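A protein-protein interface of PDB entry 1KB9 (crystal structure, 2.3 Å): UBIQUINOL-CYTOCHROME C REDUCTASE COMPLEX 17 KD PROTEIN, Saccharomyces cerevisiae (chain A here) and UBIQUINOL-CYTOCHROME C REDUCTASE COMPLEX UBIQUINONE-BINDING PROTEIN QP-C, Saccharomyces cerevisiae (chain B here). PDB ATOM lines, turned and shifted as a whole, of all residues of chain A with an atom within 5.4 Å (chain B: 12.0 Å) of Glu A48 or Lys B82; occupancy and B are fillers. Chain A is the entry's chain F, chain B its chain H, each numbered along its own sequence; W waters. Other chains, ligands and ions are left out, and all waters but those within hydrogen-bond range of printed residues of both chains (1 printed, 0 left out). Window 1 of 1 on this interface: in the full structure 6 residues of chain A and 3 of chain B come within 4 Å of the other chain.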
ATOM      1  N   CYS A  28     -13.800  -1.175 -26.397  1.00  0.00           N
ATOM      2  CA  CYS A  28     -12.554  -1.334 -25.658  1.00  0.00           C
ATOM      3  C   CYS A  28     -12.602  -0.506 -24.381  1.00  0.00           C
ATOM      4  O   CYS A  28     -12.218  -0.981 -23.316  1.00  0.00           O
ATOM      5  CB  CYS A  28     -11.351  -0.898 -26.505  1.00  0.00           C
ATOM      6  SG  CYS A  28      -9.731  -1.121 -25.685  1.00  0.00           S
ATOM      7  N   ARG A  31     -14.782  -2.169 -21.728  1.00  0.00           N
ATOM      8  CA  ARG A  31     -14.058  -3.294 -21.149  1.00  0.00           C
ATOM      9  C   ARG A  31     -12.983  -2.851 -20.153  1.00  0.00           C
ATOM     10  O   ARG A  31     -12.712  -3.545 -19.176  1.00  0.00           O
ATOM     11  CB  ARG A  31     -13.444  -4.135 -22.277  1.00  0.00           C
ATOM     12  CG  ARG A  31     -12.675  -5.367 -21.822  1.00  0.00           C
ATOM     13  CD  ARG A  31     -12.314  -6.278 -22.997  1.00  0.00           C
ATOM     14  NE  ARG A  31     -11.426  -5.643 -23.970  1.00  0.00           N
ATOM     15  CZ  ARG A  31     -11.777  -5.320 -25.214  1.00  0.00           C
ATOM     16  NH1 ARG A  31     -10.898  -4.746 -26.027  1.00  0.00           N
ATOM     17  NH2 ARG A  31     -13.010  -5.561 -25.645  1.00  0.00           N
ATOM     18  N   VAL A  32     -12.417  -1.667 -20.376  1.00  0.00           N
ATOM     19  CA  VAL A  32     -11.369  -1.135 -19.509  1.00  0.00           C
ATOM     20  C   VAL A  32     -11.851  -0.620 -18.153  1.00  0.00           C
ATOM     21  O   VAL A  32     -11.277  -0.976 -17.125  1.00  0.00           O
ATOM     22  CB  VAL A  32     -10.553  -0.029 -20.220  1.00  0.00           C
ATOM     23  CG1 VAL A  32      -9.529   0.580 -19.267  1.00  0.00           C
ATOM     24  CG2 VAL A  32      -9.843  -0.608 -21.427  1.00  0.00           C
ATOM     25  N   GLN A  35     -12.586  -3.262 -15.622  1.00  0.00           N
ATOM     26  CA  GLN A  35     -11.411  -3.882 -15.014  1.00  0.00           C
ATOM     27  C   GLN A  35     -10.814  -3.022 -13.901  1.00  0.00           C
ATOM     28  O   GLN A  35     -10.163  -3.540 -12.991  1.00  0.00           O
ATOM     29  CB  GLN A  35     -10.336  -4.148 -16.074  1.00  0.00           C
ATOM     30  CG  GLN A  35     -10.724  -5.157 -17.145  1.00  0.00           C
ATOM     31  CD  GLN A  35      -9.611  -5.394 -18.155  1.00  0.00           C
ATOM     32  OE1 GLN A  35      -8.457  -5.023 -17.927  1.00  0.00           O
ATOM     33  NE2 GLN A  35      -9.953  -6.018 -19.276  1.00  0.00           N
ATOM     34  N   TYR A  41      -6.608  -3.964  -9.063  1.00  0.00           N
ATOM     35  CA  TYR A  41      -6.245  -3.309 -10.314  1.00  0.00           C
ATOM     36  C   TYR A  41      -4.867  -2.658 -10.238  1.00  0.00           C
ATOM     37  O   TYR A  41      -4.113  -2.684 -11.210  1.00  0.00           O
ATOM     38  CB  TYR A  41      -7.295  -2.266 -10.709  1.00  0.00           C
ATOM     39  CG  TYR A  41      -7.003  -1.582 -12.028  1.00  0.00           C
ATOM     40  CD1 TYR A  41      -6.622  -0.241 -12.070  1.00  0.00           C
ATOM     41  CD2 TYR A  41      -7.088  -2.280 -13.233  1.00  0.00           C
ATOM     42  CE1 TYR A  41      -6.331   0.387 -13.277  1.00  0.00           C
ATOM     43  CE2 TYR A  41      -6.799  -1.662 -14.446  1.00  0.00           C
ATOM     44  CZ  TYR A  41      -6.420  -0.329 -14.460  1.00  0.00           C
ATOM     45  OH  TYR A  41      -6.130   0.291 -15.654  1.00  0.00           O
ATOM     46  N   HIS A  46      -0.708  -6.072 -16.026  1.00  0.00           N
ATOM     47  CA  HIS A  46      -1.299  -6.567 -17.265  1.00  0.00           C
ATOM     48  C   HIS A  46      -2.499  -5.693 -17.642  1.00  0.00           C
ATOM     49  O   HIS A  46      -3.455  -6.163 -18.262  1.00  0.00           O
ATOM     50  CB  HIS A  46      -1.743  -8.021 -17.066  1.00  0.00           C
ATOM     51  CG  HIS A  46      -1.586  -8.877 -18.283  1.00  0.00           C
ATOM     52  ND1 HIS A  46      -2.496  -8.875 -19.319  1.00  0.00           N
ATOM     53  CD2 HIS A  46      -0.635  -9.780 -18.620  1.00  0.00           C
ATOM     54  CE1 HIS A  46      -2.112  -9.741 -20.241  1.00  0.00           C
ATOM     55  NE2 HIS A  46      -0.986 -10.303 -19.841  1.00  0.00           N
ATOM     56  N   LYS A  47      -2.429  -4.418 -17.265  1.00  0.00           N
ATOM     57  CA  LYS A  47      -3.491  -3.452 -17.535  1.00  0.00           C
ATOM     58  C   LYS A  47      -3.602  -3.154 -19.026  1.00  0.00           C
ATOM     59  O   LYS A  47      -2.624  -2.779 -19.674  1.00  0.00           O
ATOM     60  CB  LYS A  47      -3.238  -2.146 -16.776  1.00  0.00           C
ATOM     61  CG  LYS A  47      -2.755  -2.325 -15.342  1.00  0.00           C
ATOM     62  CD  LYS A  47      -2.548  -0.981 -14.657  1.00  0.00           C
ATOM     63  CE  LYS A  47      -1.532  -1.077 -13.524  1.00  0.00           C
ATOM     64  NZ  LYS A  47      -1.881  -2.113 -12.516  1.00  0.00           N
ATOM     65  N   GLU A  48      -4.801  -3.326 -19.564  1.00  0.00           N
ATOM     66  CA  GLU A  48      -5.057  -3.079 -20.973  1.00  0.00           C
ATOM     67  C   GLU A  48      -5.472  -1.629 -21.208  1.00  0.00           C
ATOM     68  O   GLU A  48      -6.155  -1.027 -20.378  1.00  0.00           O
ATOM     69  CB  GLU A  48      -6.160  -4.018 -21.471  1.00  0.00           C
ATOM     70  CG  GLU A  48      -6.560  -3.815 -22.931  1.00  0.00           C
ATOM     71  CD  GLU A  48      -7.731  -4.687 -23.359  1.00  0.00           C
ATOM     72  OE1 GLU A  48      -8.383  -5.297 -22.484  1.00  0.00           O
ATOM     73  OE2 GLU A  48      -8.007  -4.760 -24.575  1.00  0.00           O
ATOM     74  N   ASP A  49      -5.007  -1.061 -22.318  1.00  0.00           N
ATOM     75  CA  ASP A  49      -5.363   0.302 -22.692  1.00  0.00           C
ATOM     76  C   ASP A  49      -5.985   0.243 -24.076  1.00  0.00           C
ATOM     77  O   ASP A  49      -5.976  -0.804 -24.714  1.00  0.00           O
ATOM     78  CB  ASP A  49      -4.152   1.245 -22.664  1.00  0.00           C
ATOM     79  CG  ASP A  49      -3.040   0.816 -23.605  1.00  0.00           C
ATOM     80  OD1 ASP A  49      -1.952   0.478 -23.093  1.00  0.00           O
ATOM     81  OD2 ASP A  49      -3.239   0.841 -24.843  1.00  0.00           O
ATOM     82  N   CYS A  50      -6.508   1.365 -24.551  1.00  0.00           N
ATOM     83  CA  CYS A  50      -7.150   1.381 -25.856  1.00  0.00           C
ATOM     84  C   CYS A  50      -6.471   2.278 -26.897  1.00  0.00           C
ATOM     85  O   CYS A  50      -7.113   2.743 -27.851  1.00  0.00           O
ATOM     86  CB  CYS A  50      -8.635   1.724 -25.687  1.00  0.00           C
ATOM     87  SG  CYS A  50      -9.501   0.565 -24.567  1.00  0.00           S
ATOM     88  N   GLU A  52      -4.311   1.434 -29.215  1.00  0.00           N
ATOM     89  CA  GLU A  52      -4.379   0.779 -30.512  1.00  0.00           C
ATOM     90  C   GLU A  52      -5.686   1.100 -31.224  1.00  0.00           C
ATOM     91  O   GLU A  52      -5.674   1.617 -32.341  1.00  0.00           O
ATOM     92  CB  GLU A  52      -4.206  -0.728 -30.339  1.00  0.00           C
ATOM     93  CG  GLU A  52      -4.133  -1.504 -31.637  1.00  0.00           C
ATOM     94  CD  GLU A  52      -3.564  -2.901 -31.447  1.00  0.00           C
ATOM     95  OE1 GLU A  52      -4.135  -3.854 -32.016  1.00  0.00           O
ATOM     96  OE2 GLU A  52      -2.542  -3.049 -30.738  1.00  0.00           O
ATOM     97  N   GLU A  53      -6.811   0.826 -30.562  1.00  0.00           N
ATOM     98  CA  GLU A  53      -8.133   1.103 -31.128  1.00  0.00           C
ATOM     99  C   GLU A  53      -8.267   2.596 -31.410  1.00  0.00           C
ATOM    100  O   GLU A  53      -8.857   2.995 -32.414  1.00  0.00           O
ATOM    101  CB  GLU A  53      -9.247   0.651 -30.176  1.00  0.00           C
ATOM    102  CG  GLU A  53      -9.380  -0.864 -30.006  1.00  0.00           C
ATOM    103  CD  GLU A  53      -8.323  -1.471 -29.095  1.00  0.00           C
ATOM    104  OE1 GLU A  53      -7.620  -0.720 -28.382  1.00  0.00           O
ATOM    105  OE2 GLU A  53      -8.206  -2.715 -29.079  1.00  0.00           O
ATOM    106  N   GLU B  74       6.331  -7.950 -41.113  1.00  0.00           N
ATOM    107  CA  GLU B  74       4.937  -8.195 -40.771  1.00  0.00           C
ATOM    108  C   GLU B  74       4.824  -8.987 -39.484  1.00  0.00           C
ATOM    109  O   GLU B  74       3.866  -8.825 -38.728  1.00  0.00           O
ATOM    110  CB  GLU B  74       4.240  -8.931 -41.908  1.00  0.00           C
ATOM    111  CG  GLU B  74       4.213  -8.119 -43.191  1.00  0.00           C
ATOM    112  CD  GLU B  74       3.548  -8.844 -44.343  1.00  0.00           C
ATOM    113  OE1 GLU B  74       2.766  -8.198 -45.076  1.00  0.00           O
ATOM    114  OE2 GLU B  74       3.814 -10.052 -44.525  1.00  0.00           O
ATOM    115  N   TYR B  75       5.817  -9.827 -39.226  1.00  0.00           N
ATOM    116  CA  TYR B  75       5.831 -10.626 -38.015  1.00  0.00           C
ATOM    117  C   TYR B  75       6.126  -9.724 -36.818  1.00  0.00           C
ATOM    118  O   TYR B  75       5.550  -9.898 -35.742  1.00  0.00           O
ATOM    119  CB  TYR B  75       6.875 -11.742 -38.130  1.00  0.00           C
ATOM    120  CG  TYR B  75       6.964 -12.646 -36.923  1.00  0.00           C
ATOM    121  CD1 TYR B  75       5.826 -13.265 -36.394  1.00  0.00           C
ATOM    122  CD2 TYR B  75       8.191 -12.884 -36.302  1.00  0.00           C
ATOM    123  CE1 TYR B  75       5.911 -14.102 -35.269  1.00  0.00           C
ATOM    124  CE2 TYR B  75       8.290 -13.713 -35.184  1.00  0.00           C
ATOM    125  CZ  TYR B  75       7.148 -14.316 -34.673  1.00  0.00           C
ATOM    126  OH  TYR B  75       7.260 -15.127 -33.569  1.00  0.00           O
ATOM    127  N   ASN B  76       7.007  -8.747 -37.020  1.00  0.00           N
ATOM    128  CA  ASN B  76       7.385  -7.812 -35.964  1.00  0.00           C
ATOM    129  C   ASN B  76       6.185  -6.936 -35.601  1.00  0.00           C
ATOM    130  O   ASN B  76       5.964  -6.620 -34.430  1.00  0.00           O
ATOM    131  CB  ASN B  76       8.567  -6.939 -36.427  1.00  0.00           C
ATOM    132  CG  ASN B  76       9.026  -5.945 -35.364  1.00  0.00           C
ATOM    133  OD1 ASN B  76       8.641  -4.779 -35.380  1.00  0.00           O
ATOM    134  ND2 ASN B  76       9.852  -6.403 -34.444  1.00  0.00           N
ATOM    135  N   GLU B  77       5.417  -6.556 -36.620  1.00  0.00           N
ATOM    136  CA  GLU B  77       4.237  -5.723 -36.449  1.00  0.00           C
ATOM    137  C   GLU B  77       3.214  -6.488 -35.607  1.00  0.00           C
ATOM    138  O   GLU B  77       2.618  -5.937 -34.678  1.00  0.00           O
ATOM    139  CB  GLU B  77       3.662  -5.362 -37.817  1.00  0.00           C
ATOM    140  CG  GLU B  77       2.783  -4.122 -37.822  1.00  0.00           C
ATOM    141  CD  GLU B  77       2.421  -3.672 -39.233  1.00  0.00           C
ATOM    142  OE1 GLU B  77       3.329  -3.197 -39.956  1.00  0.00           O
ATOM    143  OE2 GLU B  77       1.234  -3.800 -39.620  1.00  0.00           O
ATOM    144  N   PHE B  78       3.048  -7.771 -35.907  1.00  0.00           N
ATOM    145  CA  PHE B  78       2.125  -8.609 -35.154  1.00  0.00           C
ATOM    146  C   PHE B  78       2.574  -8.707 -33.691  1.00  0.00           C
ATOM    147  O   PHE B  78       1.789  -8.470 -32.780  1.00  0.00           O
ATOM    148  CB  PHE B  78       2.044 -10.002 -35.784  1.00  0.00           C
ATOM    149  CG  PHE B  78       1.433 -11.046 -34.885  1.00  0.00           C
ATOM    150  CD1 PHE B  78       0.062 -11.063 -34.643  1.00  0.00           C
ATOM    151  CD2 PHE B  78       2.234 -12.025 -34.289  1.00  0.00           C
ATOM    152  CE1 PHE B  78      -0.507 -12.046 -33.818  1.00  0.00           C
ATOM    153  CE2 PHE B  78       1.677 -13.009 -33.463  1.00  0.00           C
ATOM    154  CZ  PHE B  78       0.302 -13.021 -33.228  1.00  0.00           C
ATOM    155  N   LEU B  79       3.849  -9.011 -33.474  1.00  0.00           N
ATOM    156  CA  LEU B  79       4.382  -9.144 -32.125  1.00  0.00           C
ATOM    157  C   LEU B  79       4.145  -7.930 -31.224  1.00  0.00           C
ATOM    158  O   LEU B  79       3.950  -8.077 -30.020  1.00  0.00           O
ATOM    159  CB  LEU B  79       5.877  -9.446 -32.178  1.00  0.00           C
ATOM    160  CG  LEU B  79       6.320 -10.834 -32.642  1.00  0.00           C
ATOM    161  CD1 LEU B  79       7.843 -10.890 -32.711  1.00  0.00           C
ATOM    162  CD2 LEU B  79       5.814 -11.874 -31.660  1.00  0.00           C
ATOM    163  N   TYR B  80       4.145  -6.736 -31.808  1.00  0.00           N
ATOM    164  CA  TYR B  80       3.963  -5.520 -31.029  1.00  0.00           C
ATOM    165  C   TYR B  80       2.546  -4.949 -30.987  1.00  0.00           C
ATOM    166  O   TYR B  80       2.321  -3.841 -30.495  1.00  0.00           O
ATOM    167  CB  TYR B  80       5.025  -4.480 -31.415  1.00  0.00           C
ATOM    168  CG  TYR B  80       6.390  -4.856 -30.873  1.00  0.00           C
ATOM    169  CD1 TYR B  80       7.244  -5.691 -31.595  1.00  0.00           C
ATOM    170  CD2 TYR B  80       6.789  -4.456 -29.594  1.00  0.00           C
ATOM    171  CE1 TYR B  80       8.455  -6.129 -31.054  1.00  0.00           C
ATOM    172  CE2 TYR B  80       7.990  -4.882 -29.048  1.00  0.00           C
ATOM    173  CZ  TYR B  80       8.817  -5.720 -29.782  1.00  0.00           C
ATOM    174  OH  TYR B  80      10.003  -6.152 -29.240  1.00  0.00           O
ATOM    175  N   SER B  81       1.592  -5.728 -31.488  1.00  0.00           N
ATOM    176  CA  SER B  81       0.181  -5.352 -31.461  1.00  0.00           C
ATOM    177  C   SER B  81      -0.430  -6.088 -30.262  1.00  0.00           C
ATOM    178  O   SER B  81       0.236  -6.920 -29.634  1.00  0.00           O
ATOM    179  CB  SER B  81      -0.520  -5.783 -32.752  1.00  0.00           C
ATOM    180  OG  SER B  81      -0.536  -7.195 -32.879  1.00  0.00           O
ATOM    181  N   LYS B  82      -1.684  -5.773 -29.933  1.00  0.00           N
ATOM    182  CA  LYS B  82      -2.370  -6.416 -28.810  1.00  0.00           C
ATOM    183  C   LYS B  82      -2.431  -7.924 -28.986  1.00  0.00           C
ATOM    184  O   LYS B  82      -2.028  -8.679 -28.099  1.00  0.00           O
ATOM    185  CB  LYS B  82      -3.798  -5.891 -28.671  1.00  0.00           C
ATOM    186  CG  LYS B  82      -3.941  -4.652 -27.818  1.00  0.00           C
ATOM    187  CD  LYS B  82      -5.411  -4.359 -27.556  1.00  0.00           C
ATOM    188  CE  LYS B  82      -5.562  -3.148 -26.669  1.00  0.00           C
ATOM    189  NZ  LYS B  82      -6.978  -2.719 -26.552  1.00  0.00           N
ATOM    190  N   ALA B  83      -2.920  -8.347 -30.149  1.00  0.00           N
ATOM    191  CA  ALA B  83      -3.073  -9.757 -30.485  1.00  0.00           C
ATOM    192  C   ALA B  83      -1.835 -10.618 -30.269  1.00  0.00           C
ATOM    193  O   ALA B  83      -1.948 -11.796 -29.917  1.00  0.00           O
ATOM    194  CB  ALA B  83      -3.557  -9.899 -31.928  1.00  0.00           C
ATOM    195  N   GLY B  84      -0.657 -10.027 -30.453  1.00  0.00           N
ATOM    196  CA  GLY B  84       0.571 -10.786 -30.308  1.00  0.00           C
ATOM    197  C   GLY B  84       1.396 -10.605 -29.053  1.00  0.00           C
ATOM    198  O   GLY B  84       2.490 -11.162 -28.973  1.00  0.00           O
ATOM    199  N   ARG B  85       0.887  -9.871 -28.067  1.00  0.00           N
ATOM    200  CA  ARG B  85       1.643  -9.645 -26.836  1.00  0.00           C
ATOM    201  C   ARG B  85       1.902 -10.927 -26.056  1.00  0.00           C
ATOM    202  O   ARG B  85       2.805 -10.986 -25.220  1.00  0.00           O
ATOM    203  CB  ARG B  85       0.963  -8.603 -25.938  1.00  0.00           C
ATOM    204  CG  ARG B  85      -0.398  -9.003 -25.404  1.00  0.00           C
ATOM    205  CD  ARG B  85      -0.795  -8.135 -24.215  1.00  0.00           C
ATOM    206  NE  ARG B  85       0.211  -8.182 -23.152  1.00  0.00           N
ATOM    207  CZ  ARG B  85       0.552  -9.279 -22.476  1.00  0.00           C
ATOM    208  NH1 ARG B  85       1.485  -9.212 -21.533  1.00  0.00           N
ATOM    209  NH2 ARG B  85      -0.046 -10.440 -22.728  1.00  0.00           N
ATOM    210  N   GLU B  86       1.108 -11.953 -26.341  1.00  0.00           N
ATOM    211  CA  GLU B  86       1.249 -13.245 -25.682  1.00  0.00           C
ATOM    212  C   GLU B  86       2.456 -13.951 -26.301  1.00  0.00           C
ATOM    213  O   GLU B  86       3.342 -14.423 -25.588  1.00  0.00           O
ATOM    214  CB  GLU B  86      -0.032 -14.064 -25.868  1.00  0.00           C
ATOM    215  CG  GLU B  86      -0.229 -15.161 -24.835  1.00  0.00           C
ATOM    216  CD  GLU B  86      -1.629 -15.751 -24.875  1.00  0.00           C
ATOM    217  OE1 GLU B  86      -1.920 -16.543 -25.801  1.00  0.00           O
ATOM    218  OE2 GLU B  86      -2.438 -15.417 -23.980  1.00  0.00           O
ATOM    219  N   GLU B  87       2.494 -13.976 -27.634  1.00  0.00           N
ATOM    220  CA  GLU B  87       3.595 -14.579 -28.380  1.00  0.00           C
ATOM    221  C   GLU B  87       4.890 -13.798 -28.141  1.00  0.00           C
ATOM    222  O   GLU B  87       5.973 -14.379 -28.100  1.00  0.00           O
ATOM    223  CB  GLU B  87       3.273 -14.607 -29.877  1.00  0.00           C
ATOM    224  CG  GLU B  87       4.467 -14.952 -30.757  1.00  0.00           C
ATOM    225  CD  GLU B  87       4.238 -16.170 -31.624  1.00  0.00           C
ATOM    226  OE1 GLU B  87       4.028 -16.000 -32.845  1.00  0.00           O
ATOM    227  OE2 GLU B  87       4.283 -17.297 -31.085  1.00  0.00           O
ATOM    228  N   LEU B  88       4.763 -12.482 -27.973  1.00  0.00           N
ATOM    229  CA  LEU B  88       5.906 -11.604 -27.726  1.00  0.00           C
ATOM    230  C   LEU B  88       6.656 -12.042 -26.472  1.00  0.00           C
ATOM    231  O   LEU B  88       7.867 -12.213 -26.511  1.00  0.00           O
ATOM    232  CB  LEU B  88       5.441 -10.141 -27.607  1.00  0.00           C
ATOM    233  CG  LEU B  88       6.420  -8.960 -27.488  1.00  0.00           C
ATOM    234  CD1 LEU B  88       6.934  -8.791 -26.068  1.00  0.00           C
ATOM    235  CD2 LEU B  88       7.564  -9.118 -28.465  1.00  0.00           C
ATOM    236  N   GLU B  89       5.935 -12.253 -25.374  1.00  0.00           N
ATOM    237  CA  GLU B  89       6.563 -12.681 -24.123  1.00  0.00           C
ATOM    238  C   GLU B  89       7.254 -14.032 -24.271  1.00  0.00           C
ATOM    239  O   GLU B  89       8.239 -14.314 -23.592  1.00  0.00           O
ATOM    240  CB  GLU B  89       5.536 -12.760 -22.991  1.00  0.00           C
ATOM    241  CG  GLU B  89       5.185 -11.424 -22.361  1.00  0.00           C
ATOM    242  CD  GLU B  89       4.627 -11.577 -20.951  1.00  0.00           C
ATOM    243  OE1 GLU B  89       5.434 -11.587 -19.990  1.00  0.00           O
ATOM    244  OE2 GLU B  89       3.387 -11.692 -20.806  1.00  0.00           O
ATOM    245  N   ARG B  90       6.730 -14.848 -25.178  1.00  0.00           N
ATOM    246  CA  ARG B  90       7.262 -16.174 -25.447  1.00  0.00           C
ATOM    247  C   ARG B  90       8.587 -16.131 -26.221  1.00  0.00           C
ATOM    248  O   ARG B  90       9.598 -16.660 -25.755  1.00  0.00           O
ATOM    249  CB  ARG B  90       6.219 -16.986 -26.220  1.00  0.00           C
ATOM    250  CG  ARG B  90       6.565 -18.454 -26.453  1.00  0.00           C
ATOM    251  CD  ARG B  90       5.458 -19.151 -27.240  1.00  0.00           C
ATOM    252  NE  ARG B  90       4.163 -19.049 -26.566  1.00  0.00           N
ATOM    253  CZ  ARG B  90       3.035 -18.643 -27.148  1.00  0.00           C
ATOM    254  NH1 ARG B  90       1.913 -18.584 -26.443  1.00  0.00           N
ATOM    255  NH2 ARG B  90       3.025 -18.297 -28.432  1.00  0.00           N
HETATM  256  O   HOH W   1      -3.994  -6.625 -32.091  1.00  0.00           O
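Glu A52 touches Ser B81 (OE2 to CA, 3.6 Å).
SG of Cys A28 is in hydrogen-bond range of NZ of Lys B82, at 3.3 Å.
A ring nitrogen (NE2) of His A46 sits at hydrogen-bond distance from the guanidinium group of Arg B85 (3.0 Å).
The side-chain amino group (NZ) of Lys B82 is in salt-bridge range of the side-chain carboxylate (OE2) of Glu A48, at 3.0 Å.
The side-chain amino group (NZ) of Lys B82 is in hydrogen-bond range of the backbone carbonyl oxygen (O) of Asp A49, 2.8 Å away.
The side-chain carboxylate (OE2) of Glu A52 sits at hydrogen-bond distance from the backbone NH (N) of Lys B82 (3.0 Å).
The side-chain amino group of Lys B82 lies within salt-bridge range of the side-chain carboxylate of Glu A53.
The side-chain sulfur (SG) of Cys A28 forms a disulfide with the side-chain sulfur (SG) of Cys A50, 2.0 Å away.
NH1 of Arg A31 is in salt-bridge range of OE2 of Glu A48 (3.2 Å).
OG of Ser B81 sits at hydrogen-bond distance from O of Phe B78.
The side-chain carboxylate of Glu B89 is in salt-bridge range of the guanidinium group of Arg B85 (3.2 Å).
Water W1 lies within hydrogen-bond range of the side-chain carboxylate (OE1) of Glu A52, the backbone NH (N) of Ala B83 and the backbone NH (N) of Lys B82.
Of chain B, only Lys B82 comes within 4 Å of Glu A48.
Lys B82 touches five residues of chain A.
Val A32 touches none of the printed residues of chain B.
No residue of chain B comes within 4 Å of Lys A47.
Of chain B, only Lys B82 (2.8 Å) comes within 4 Å of Asp A49.
No residue of chain B comes within 4 Å of Cys A50.
Of chain B, only Ser B81 (3.6 Å) and Lys B82 (3.0 Å) come within 4 Å of Glu A52.
Of the printed residues of chain A, Arg B85 touches His A46 (3.0 Å).
Of the printed residues of chain A, Ser B81 touches Glu A52.
Printed residues of chain B within 4 Å of Glu A53: Lys B82.
Of the printed residues of chain B, His A46 touches Arg B85.
The nearest residue of chain A that does not touch Lys B82 is Cys A50 (4.2 Å).
Of the 17 printed residues of chain B, 3 touch a printed residue of chain A.
Hydrophobic or aromatic side chains of chain A that line the printed part of chain B: His A46.
Among the printed residues, Asp or Glu carboxylates within 4 Å of a Lys or Arg side-chain nitrogen of the other chain: Glu A48 with Lys B82 (3.0 Å) and Glu A53 with Lys B82 (2.8 Å).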
